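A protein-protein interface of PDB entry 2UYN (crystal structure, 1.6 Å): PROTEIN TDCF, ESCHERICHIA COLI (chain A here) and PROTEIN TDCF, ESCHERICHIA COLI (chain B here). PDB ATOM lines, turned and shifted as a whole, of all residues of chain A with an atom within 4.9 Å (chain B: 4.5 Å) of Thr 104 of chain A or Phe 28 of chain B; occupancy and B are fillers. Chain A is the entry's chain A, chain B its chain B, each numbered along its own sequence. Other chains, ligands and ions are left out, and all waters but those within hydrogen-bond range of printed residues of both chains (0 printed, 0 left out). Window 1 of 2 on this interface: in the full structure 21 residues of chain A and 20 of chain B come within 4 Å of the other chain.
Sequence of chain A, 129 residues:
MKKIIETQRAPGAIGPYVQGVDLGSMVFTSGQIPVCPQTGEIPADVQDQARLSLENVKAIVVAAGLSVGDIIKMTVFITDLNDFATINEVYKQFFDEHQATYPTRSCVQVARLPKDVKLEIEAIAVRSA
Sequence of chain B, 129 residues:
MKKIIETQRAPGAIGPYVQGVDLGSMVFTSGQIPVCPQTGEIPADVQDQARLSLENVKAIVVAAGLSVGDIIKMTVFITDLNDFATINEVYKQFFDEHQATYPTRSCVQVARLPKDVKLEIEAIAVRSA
Tyr 91 of chain A touches none of the printed residues of chain B.
Thr 104 of chain A touches just these residues of chain B: Val 18, Gly 20, Val 21, Phe 28 and Ser 30.
Of the printed residues of chain B, Arg 105 of chain A touches Ser 30 (2.8 Å).
Printed residues of chain B within 4 Å of Ile 124 of chain A: Phe 28 (3.9 Å).
Printed residues of chain A within 4 Å of Val 18 of chain B: Tyr 102 (3.4 Å), Pro 103 (3.3 Å) and Thr 104 (3.8 Å).
Of the printed residues of chain A, Gly 20 of chain B touches Thr 104.
Phe 28 of chain B touches just these residues of chain A: Ile 72 (3.9 Å), Thr 104 (3.6 Å) and Ile 124 (3.9 Å).
Of the printed residues of chain A, Ser 30 of chain B touches Thr 104 and Arg 105.
Ala 123 of chain B touches none of the printed residues of chain A.
The nearest printed residue of chain A that does not touch Gly 20 of chain B is Ile 72 of chain A (6.5 Å).
The backbone carbonyl oxygen (O) of Ile 72 of chain A sits at hydrogen-bond distance from the side-chain hydroxyl (OG1) of Thr 104 of chain A (2.8 Å).
N of Ile 72 of chain A is in hydrogen-bond range of O of Ile 124 of chain A (2.8 Å).
The backbone NH of Ile 124 of chain A is in hydrogen-bond range of the backbone carbonyl oxygen of Lys 73 of chain A (2.9 Å).
The backbone carbonyl oxygen (O) of Thr 104 of chain A sits at hydrogen-bond distance from the backbone NH (N) of Met 74 of chain A, 3.0 Å away.
N of Ser 30 of chain B lies within hydrogen-bond range of O of Gln 19 of chain B, 2.9 Å away.
The backbone NH of Val 21 of chain B lies within hydrogen-bond range of the backbone carbonyl oxygen of Phe 28 of chain B (2.9 Å).
Among the printed residues, pairs that only touch across the chains: Ile 72 of chain A with Phe 28 of chain B (3.9 Å), Tyr 102 of chain A with Val 18 of chain B (3.4 Å), Thr 104 of chain A with Val 18 of chain B (3.8 Å), Thr 104 of chain A with Gly 20 of chain B (3.5 Å), Thr 104 of chain A with Val 21 of chain B (3.5 Å), Thr 104 of chain A with Phe 28 of chain B (3.6 Å), Thr 104 of chain A with Ser 30 of chain B (3.3 Å) and Ile 124 of chain A with Phe 28 of chain B (3.9 Å).
Of the 10 printed residues of chain A, 6 touch a printed residue of chain B.
Hydrophobic or aromatic side chains of chain A within 4 Å of the printed part of chain B: Ile 72 and Ile 124.
Printed residues of chain B that touch a printed residue of chain A: Val 18, Gly 20, Val 21, Phe 28 and Ser 30.
Hydrophobic or aromatic side chains of chain B within 4 Å of the printed part of chain A: Val 18, Val 21 and Phe 28.
Among the printed residues, 10 pairs touch across the chains.
The backbone carbonyl oxygen (O) of Pro 103 of chain A is in hydrogen-bond range of the backbone NH (N) of Val 18 of chain B, at 3.3 Å.
N of Arg 105 of chain A sits at hydrogen-bond distance from OG of Ser 30 of chain B (2.8 Å).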
ATOM      1  N   ILE A  72       6.426  -0.489  26.372  1.00  0.00           N
ATOM      2  CA  ILE A  72       7.101  -1.789  26.285  1.00  0.00           C
ATOM      3  C   ILE A  72       6.346  -2.808  25.432  1.00  0.00           C
ATOM      4  O   ILE A  72       6.923  -3.788  25.035  1.00  0.00           O
ATOM      5  CB  ILE A  72       7.469  -2.330  27.697  1.00  0.00           C
ATOM      6  CG1 ILE A  72       6.254  -2.358  28.626  1.00  0.00           C
ATOM      7  CG2 ILE A  72       8.523  -1.402  28.319  1.00  0.00           C
ATOM      8  CD1 ILE A  72       5.350  -3.561  28.490  1.00  0.00           C
ATOM      9  N   LYS A  73       5.059  -2.561  25.169  1.00  0.00           N
ATOM     10  CA  LYS A  73       4.287  -3.473  24.294  1.00  0.00           C
ATOM     11  C   LYS A  73       3.215  -2.679  23.571  1.00  0.00           C
ATOM     12  O   LYS A  73       2.570  -1.841  24.188  1.00  0.00           O
ATOM     13  CB  LYS A  73       3.651  -4.628  25.111  1.00  0.00           C
ATOM     14  CG  LYS A  73       2.553  -5.491  24.388  1.00  0.00           C
ATOM     15  CD  LYS A  73       3.181  -6.463  23.397  1.00  0.00           C
ATOM     16  CE  LYS A  73       2.149  -7.396  22.697  1.00  0.00           C
ATOM     17  NZ  LYS A  73       1.022  -6.729  22.000  1.00  0.00           N
ATOM     18  N   MET A  74       3.071  -2.900  22.261  1.00  0.00           N
ATOM     19  CA  MET A  74       1.943  -2.340  21.517  1.00  0.00           C
ATOM     20  C   MET A  74       1.261  -3.461  20.758  1.00  0.00           C
ATOM     21  O   MET A  74       1.903  -4.454  20.392  1.00  0.00           O
ATOM     22  CB  MET A  74       2.375  -1.279  20.498  1.00  0.00           C
ATOM     23  CG  MET A  74       3.504  -0.334  20.913  1.00  0.00           C
ATOM     24  SD  MET A  74       3.389   1.209  19.957  1.00  0.00           S
ATOM     25  CE  MET A  74       2.418   1.694  21.144  1.00  0.00           C
ATOM     26  N   TYR A  91       6.020   4.226  11.964  1.00  0.00           N
ATOM     27  CA  TYR A  91       6.230   3.705  13.323  1.00  0.00           C
ATOM     28  C   TYR A  91       7.698   3.735  13.734  1.00  0.00           C
ATOM     29  O   TYR A  91       8.021   4.182  14.857  1.00  0.00           O
ATOM     30  CB  TYR A  91       5.682   2.271  13.349  1.00  0.00           C
ATOM     31  CG  TYR A  91       5.607   1.547  14.684  1.00  0.00           C
ATOM     32  CD1 TYR A  91       6.760   1.081  15.311  1.00  0.00           C
ATOM     33  CD2 TYR A  91       4.367   1.213  15.239  1.00  0.00           C
ATOM     34  CE1 TYR A  91       6.689   0.352  16.515  1.00  0.00           C
ATOM     35  CE2 TYR A  91       4.276   0.474  16.432  1.00  0.00           C
ATOM     36  CZ  TYR A  91       5.426   0.056  17.062  1.00  0.00           C
ATOM     37  OH  TYR A  91       5.294  -0.673  18.208  1.00  0.00           O
ATOM     38  N   TYR A 102      12.570   0.140  20.445  1.00  0.00           N
ATOM     39  CA  TYR A 102      11.279  -0.381  19.957  1.00  0.00           C
ATOM     40  C   TYR A 102      10.619  -1.311  20.978  1.00  0.00           C
ATOM     41  O   TYR A 102      11.292  -2.178  21.552  1.00  0.00           O
ATOM     42  CB  TYR A 102      11.430  -1.130  18.633  1.00  0.00           C
ATOM     43  CG  TYR A 102      12.184  -0.336  17.608  1.00  0.00           C
ATOM     44  CD1 TYR A 102      11.912   1.025  17.412  1.00  0.00           C
ATOM     45  CD2 TYR A 102      13.155  -0.938  16.823  1.00  0.00           C
ATOM     46  CE1 TYR A 102      12.627   1.779  16.469  1.00  0.00           C
ATOM     47  CE2 TYR A 102      13.879  -0.191  15.893  1.00  0.00           C
ATOM     48  CZ  TYR A 102      13.595   1.163  15.712  1.00  0.00           C
ATOM     49  OH  TYR A 102      14.327   1.908  14.797  1.00  0.00           O
ATOM     50  N   PRO A 103       9.305  -1.119  21.214  1.00  0.00           N
ATOM     51  CA  PRO A 103       8.634  -2.066  22.115  1.00  0.00           C
ATOM     52  C   PRO A 103       8.434  -3.446  21.494  1.00  0.00           C
ATOM     53  O   PRO A 103       8.704  -3.640  20.304  1.00  0.00           O
ATOM     54  CB  PRO A 103       7.282  -1.409  22.428  1.00  0.00           C
ATOM     55  CG  PRO A 103       7.054  -0.396  21.394  1.00  0.00           C
ATOM     56  CD  PRO A 103       8.418  -0.027  20.761  1.00  0.00           C
ATOM     57  N   THR A 104       7.971  -4.399  22.306  1.00  0.00           N
ATOM     58  CA  THR A 104       7.418  -5.640  21.720  1.00  0.00           C
ATOM     59  C   THR A 104       6.142  -5.268  20.958  1.00  0.00           C
ATOM     60  O   THR A 104       5.495  -4.252  21.259  1.00  0.00           O
ATOM     61  CB  THR A 104       7.118  -6.700  22.777  1.00  0.00           C
ATOM     62  OG1 THR A 104       6.162  -6.194  23.733  1.00  0.00           O
ATOM     63  CG2 THR A 104       8.404  -7.090  23.457  1.00  0.00           C
ATOM     64  N   ARG A 105       5.753  -6.104  19.996  1.00  0.00           N
ATOM     65  CA  ARG A 105       4.618  -5.733  19.161  1.00  0.00           C
ATOM     66  C   ARG A 105       3.918  -6.964  18.620  1.00  0.00           C
ATOM     67  O   ARG A 105       4.572  -7.988  18.371  1.00  0.00           O
ATOM     68  CB  ARG A 105       5.093  -4.878  17.982  1.00  0.00           C
ATOM     69  CG  ARG A 105       3.980  -4.046  17.334  1.00  0.00           C
ATOM     70  CD  ARG A 105       4.556  -3.162  16.218  1.00  0.00           C
ATOM     71  NE  ARG A 105       4.873  -3.925  15.024  1.00  0.00           N
ATOM     72  CZ  ARG A 105       5.176  -3.360  13.854  1.00  0.00           C
ATOM     73  NH1 ARG A 105       5.247  -2.032  13.755  1.00  0.00           N
ATOM     74  NH2 ARG A 105       5.426  -4.123  12.785  1.00  0.00           N
ATOM     75  N   SER A 106       2.613  -6.827  18.406  1.00  0.00           N
ATOM     76  CA  SER A 106       1.846  -7.765  17.572  1.00  0.00           C
ATOM     77  C   SER A 106       1.136  -6.933  16.527  1.00  0.00           C
ATOM     78  O   SER A 106       0.701  -5.818  16.809  1.00  0.00           O
ATOM     79  CB  SER A 106       0.829  -8.551  18.411  1.00  0.00           C
ATOM     80  OG  SER A 106       1.527  -9.522  19.202  1.00  0.00           O
ATOM     81  N   ILE A 124       1.124  -0.512  26.313  1.00  0.00           N
ATOM     82  CA  ILE A 124       1.406  -0.703  27.735  1.00  0.00           C
ATOM     83  C   ILE A 124       2.789  -0.105  27.979  1.00  0.00           C
ATOM     84  O   ILE A 124       3.732  -0.346  27.217  1.00  0.00           O
ATOM     85  CB  ILE A 124       1.447  -2.201  28.082  1.00  0.00           C
ATOM     86  CG1 ILE A 124       0.136  -2.875  27.634  1.00  0.00           C
ATOM     87  CG2 ILE A 124       1.726  -2.378  29.590  1.00  0.00           C
ATOM     88  CD1 ILE A 124       0.125  -4.391  27.863  1.00  0.00           C
ATOM     89  N   VAL B  18      11.166  -5.437  19.163  1.00  0.00           N
ATOM     90  CA  VAL B  18      12.131  -6.374  19.713  1.00  0.00           C
ATOM     91  C   VAL B  18      11.419  -7.683  20.013  1.00  0.00           C
ATOM     92  O   VAL B  18      10.171  -7.699  20.135  1.00  0.00           O
ATOM     93  CB  VAL B  18      12.811  -5.808  20.965  1.00  0.00           C
ATOM     94  CG1 VAL B  18      13.595  -4.552  20.592  1.00  0.00           C
ATOM     95  CG2 VAL B  18      11.796  -5.464  22.065  1.00  0.00           C
ATOM     96  N   GLN B  19      12.179  -8.775  20.111  1.00  0.00           N
ATOM     97  CA  GLN B  19      11.539 -10.105  20.343  1.00  0.00           C
ATOM     98  C   GLN B  19      10.786 -10.198  21.659  1.00  0.00           C
ATOM     99  O   GLN B  19       9.698 -10.766  21.732  1.00  0.00           O
ATOM    100  CB  GLN B  19      12.563 -11.240  20.287  1.00  0.00           C
ATOM    101  CG  GLN B  19      13.181 -11.444  18.923  1.00  0.00           C
ATOM    102  CD  GLN B  19      14.366 -12.367  19.021  1.00  0.00           C
ATOM    103  OE1 GLN B  19      15.160 -12.283  19.975  1.00  0.00           O
ATOM    104  NE2 GLN B  19      14.487 -13.267  18.075  1.00  0.00           N
ATOM    105  N   GLY B  20      11.370  -9.672  22.732  1.00  0.00           N
ATOM    106  CA  GLY B  20      10.717  -9.744  24.026  1.00  0.00           C
ATOM    107  C   GLY B  20      11.272  -8.623  24.879  1.00  0.00           C
ATOM    108  O   GLY B  20      12.299  -7.980  24.528  1.00  0.00           O
ATOM    109  N   VAL B  21      10.566  -8.358  25.966  1.00  0.00           N
ATOM    110  CA  VAL B  21      11.046  -7.404  26.977  1.00  0.00           C
ATOM    111  C   VAL B  21      10.840  -8.030  28.350  1.00  0.00           C
ATOM    112  O   VAL B  21       9.802  -8.640  28.633  1.00  0.00           O
ATOM    113  CB  VAL B  21      10.309  -6.024  26.868  1.00  0.00           C
ATOM    114  CG1 VAL B  21      10.680  -5.094  28.035  1.00  0.00           C
ATOM    115  CG2 VAL B  21      10.681  -5.341  25.590  1.00  0.00           C
ATOM    116  N   LEU B  23      10.641  -7.183  32.302  1.00  0.00           N
ATOM    117  CA  LEU B  23      10.391  -6.068  33.212  1.00  0.00           C
ATOM    118  C   LEU B  23      10.780  -6.438  34.629  1.00  0.00           C
ATOM    119  O   LEU B  23      10.570  -5.650  35.548  1.00  0.00           O
ATOM    120  CB  LEU B  23       8.910  -5.705  33.212  1.00  0.00           C
ATOM    121  CG  LEU B  23       8.188  -5.433  31.897  1.00  0.00           C
ATOM    122  CD1 LEU B  23       6.749  -5.024  32.247  1.00  0.00           C
ATOM    123  CD2 LEU B  23       8.896  -4.369  31.061  1.00  0.00           C
ATOM    124  N   MET B  26       7.736  -9.634  35.059  1.00  0.00           N
ATOM    125  CA  MET B  26       6.921 -10.039  33.918  1.00  0.00           C
ATOM    126  C   MET B  26       7.706  -9.940  32.616  1.00  0.00           C
ATOM    127  O   MET B  26       8.494  -9.019  32.426  1.00  0.00           O
ATOM    128  CB  MET B  26       5.678  -9.136  33.855  1.00  0.00           C
ATOM    129  CG  MET B  26       4.588  -9.626  32.978  1.00  0.00           C
ATOM    130  SD  MET B  26       3.048  -8.661  33.147  1.00  0.00           S
ATOM    131  CE  MET B  26       3.538  -7.070  33.697  1.00  0.00           C
ATOM    132  N   VAL B  27       7.483 -10.908  31.722  1.00  0.00           N
ATOM    133  CA  VAL B  27       8.101 -10.895  30.387  1.00  0.00           C
ATOM    134  C   VAL B  27       6.990 -10.838  29.333  1.00  0.00           C
ATOM    135  O   VAL B  27       6.014 -11.567  29.438  1.00  0.00           O
ATOM    136  CB  VAL B  27       8.998 -12.161  30.162  1.00  0.00           C
ATOM    137  CG1 VAL B  27       9.261 -12.443  28.706  1.00  0.00           C
ATOM    138  CG2 VAL B  27      10.322 -12.057  30.977  1.00  0.00           C
ATOM    139  N   PHE B  28       7.135  -9.926  28.372  1.00  0.00           N
ATOM    140  CA  PHE B  28       6.234  -9.857  27.205  1.00  0.00           C
ATOM    141  C   PHE B  28       6.969 -10.301  25.959  1.00  0.00           C
ATOM    142  O   PHE B  28       8.101  -9.863  25.718  1.00  0.00           O
ATOM    143  CB  PHE B  28       5.769  -8.408  26.962  1.00  0.00           C
ATOM    144  CG  PHE B  28       4.762  -7.901  27.965  1.00  0.00           C
ATOM    145  CD1 PHE B  28       5.175  -7.422  29.213  1.00  0.00           C
ATOM    146  CD2 PHE B  28       3.402  -7.877  27.654  1.00  0.00           C
ATOM    147  CE1 PHE B  28       4.237  -6.947  30.138  1.00  0.00           C
ATOM    148  CE2 PHE B  28       2.456  -7.402  28.571  1.00  0.00           C
ATOM    149  CZ  PHE B  28       2.872  -6.944  29.813  1.00  0.00           C
ATOM    150  N   THR B  29       6.334 -11.138  25.134  1.00  0.00           N
ATOM    151  CA  THR B  29       6.894 -11.405  23.793  1.00  0.00           C
ATOM    152  C   THR B  29       6.127 -10.619  22.718  1.00  0.00           C
ATOM    153  O   THR B  29       4.921 -10.287  22.865  1.00  0.00           O
ATOM    154  CB  THR B  29       6.870 -12.910  23.380  1.00  0.00           C
ATOM    155  OG1 THR B  29       5.554 -13.288  22.930  1.00  0.00           O
ATOM    156  CG2 THR B  29       7.301 -13.849  24.532  1.00  0.00           C
ATOM    157  N   SER B  30       6.822 -10.343  21.619  1.00  0.00           N
ATOM    158  CA  SER B  30       6.138  -9.931  20.398  1.00  0.00           C
ATOM    159  C   SER B  30       5.319 -11.111  19.888  1.00  0.00           C
ATOM    160  O   SER B  30       5.572 -12.280  20.275  1.00  0.00           O
ATOM    161  CB  SER B  30       7.174  -9.489  19.368  1.00  0.00           C
ATOM    162  OG  SER B  30       7.645  -8.183  19.700  1.00  0.00           O
ATOM    163  N   ALA B 123       2.748 -13.874  24.034  1.00  0.00           N
ATOM    164  CA  ALA B 123       2.694 -14.428  25.363  1.00  0.00           C
ATOM    165  C   ALA B 123       3.083 -13.403  26.394  1.00  0.00           C
ATOM    166  O   ALA B 123       3.900 -12.539  26.133  1.00  0.00           O
ATOM    167  CB  ALA B 123       3.657 -15.642  25.473  1.00  0.00           C
ATOM    168  N   ILE B 124       2.549 -13.596  27.593  1.00  0.00           N
ATOM    169  CA  ILE B 124       3.004 -12.910  28.809  1.00  0.00           C
ATOM    170  C   ILE B 124       3.413 -14.018  29.811  1.00  0.00           C
ATOM    171  O   ILE B 124       2.643 -14.941  30.057  1.00  0.00           O
ATOM    172  CB  ILE B 124       1.890 -12.043  29.415  1.00  0.00           C
ATOM    173  CG1 ILE B 124       1.374 -11.034  28.373  1.00  0.00           C
ATOM    174  CG2 ILE B 124       2.424 -11.318  30.671  1.00  0.00           C
ATOM    175  CD1 ILE B 124       0.082 -10.296  28.784  1.00  0.00           C
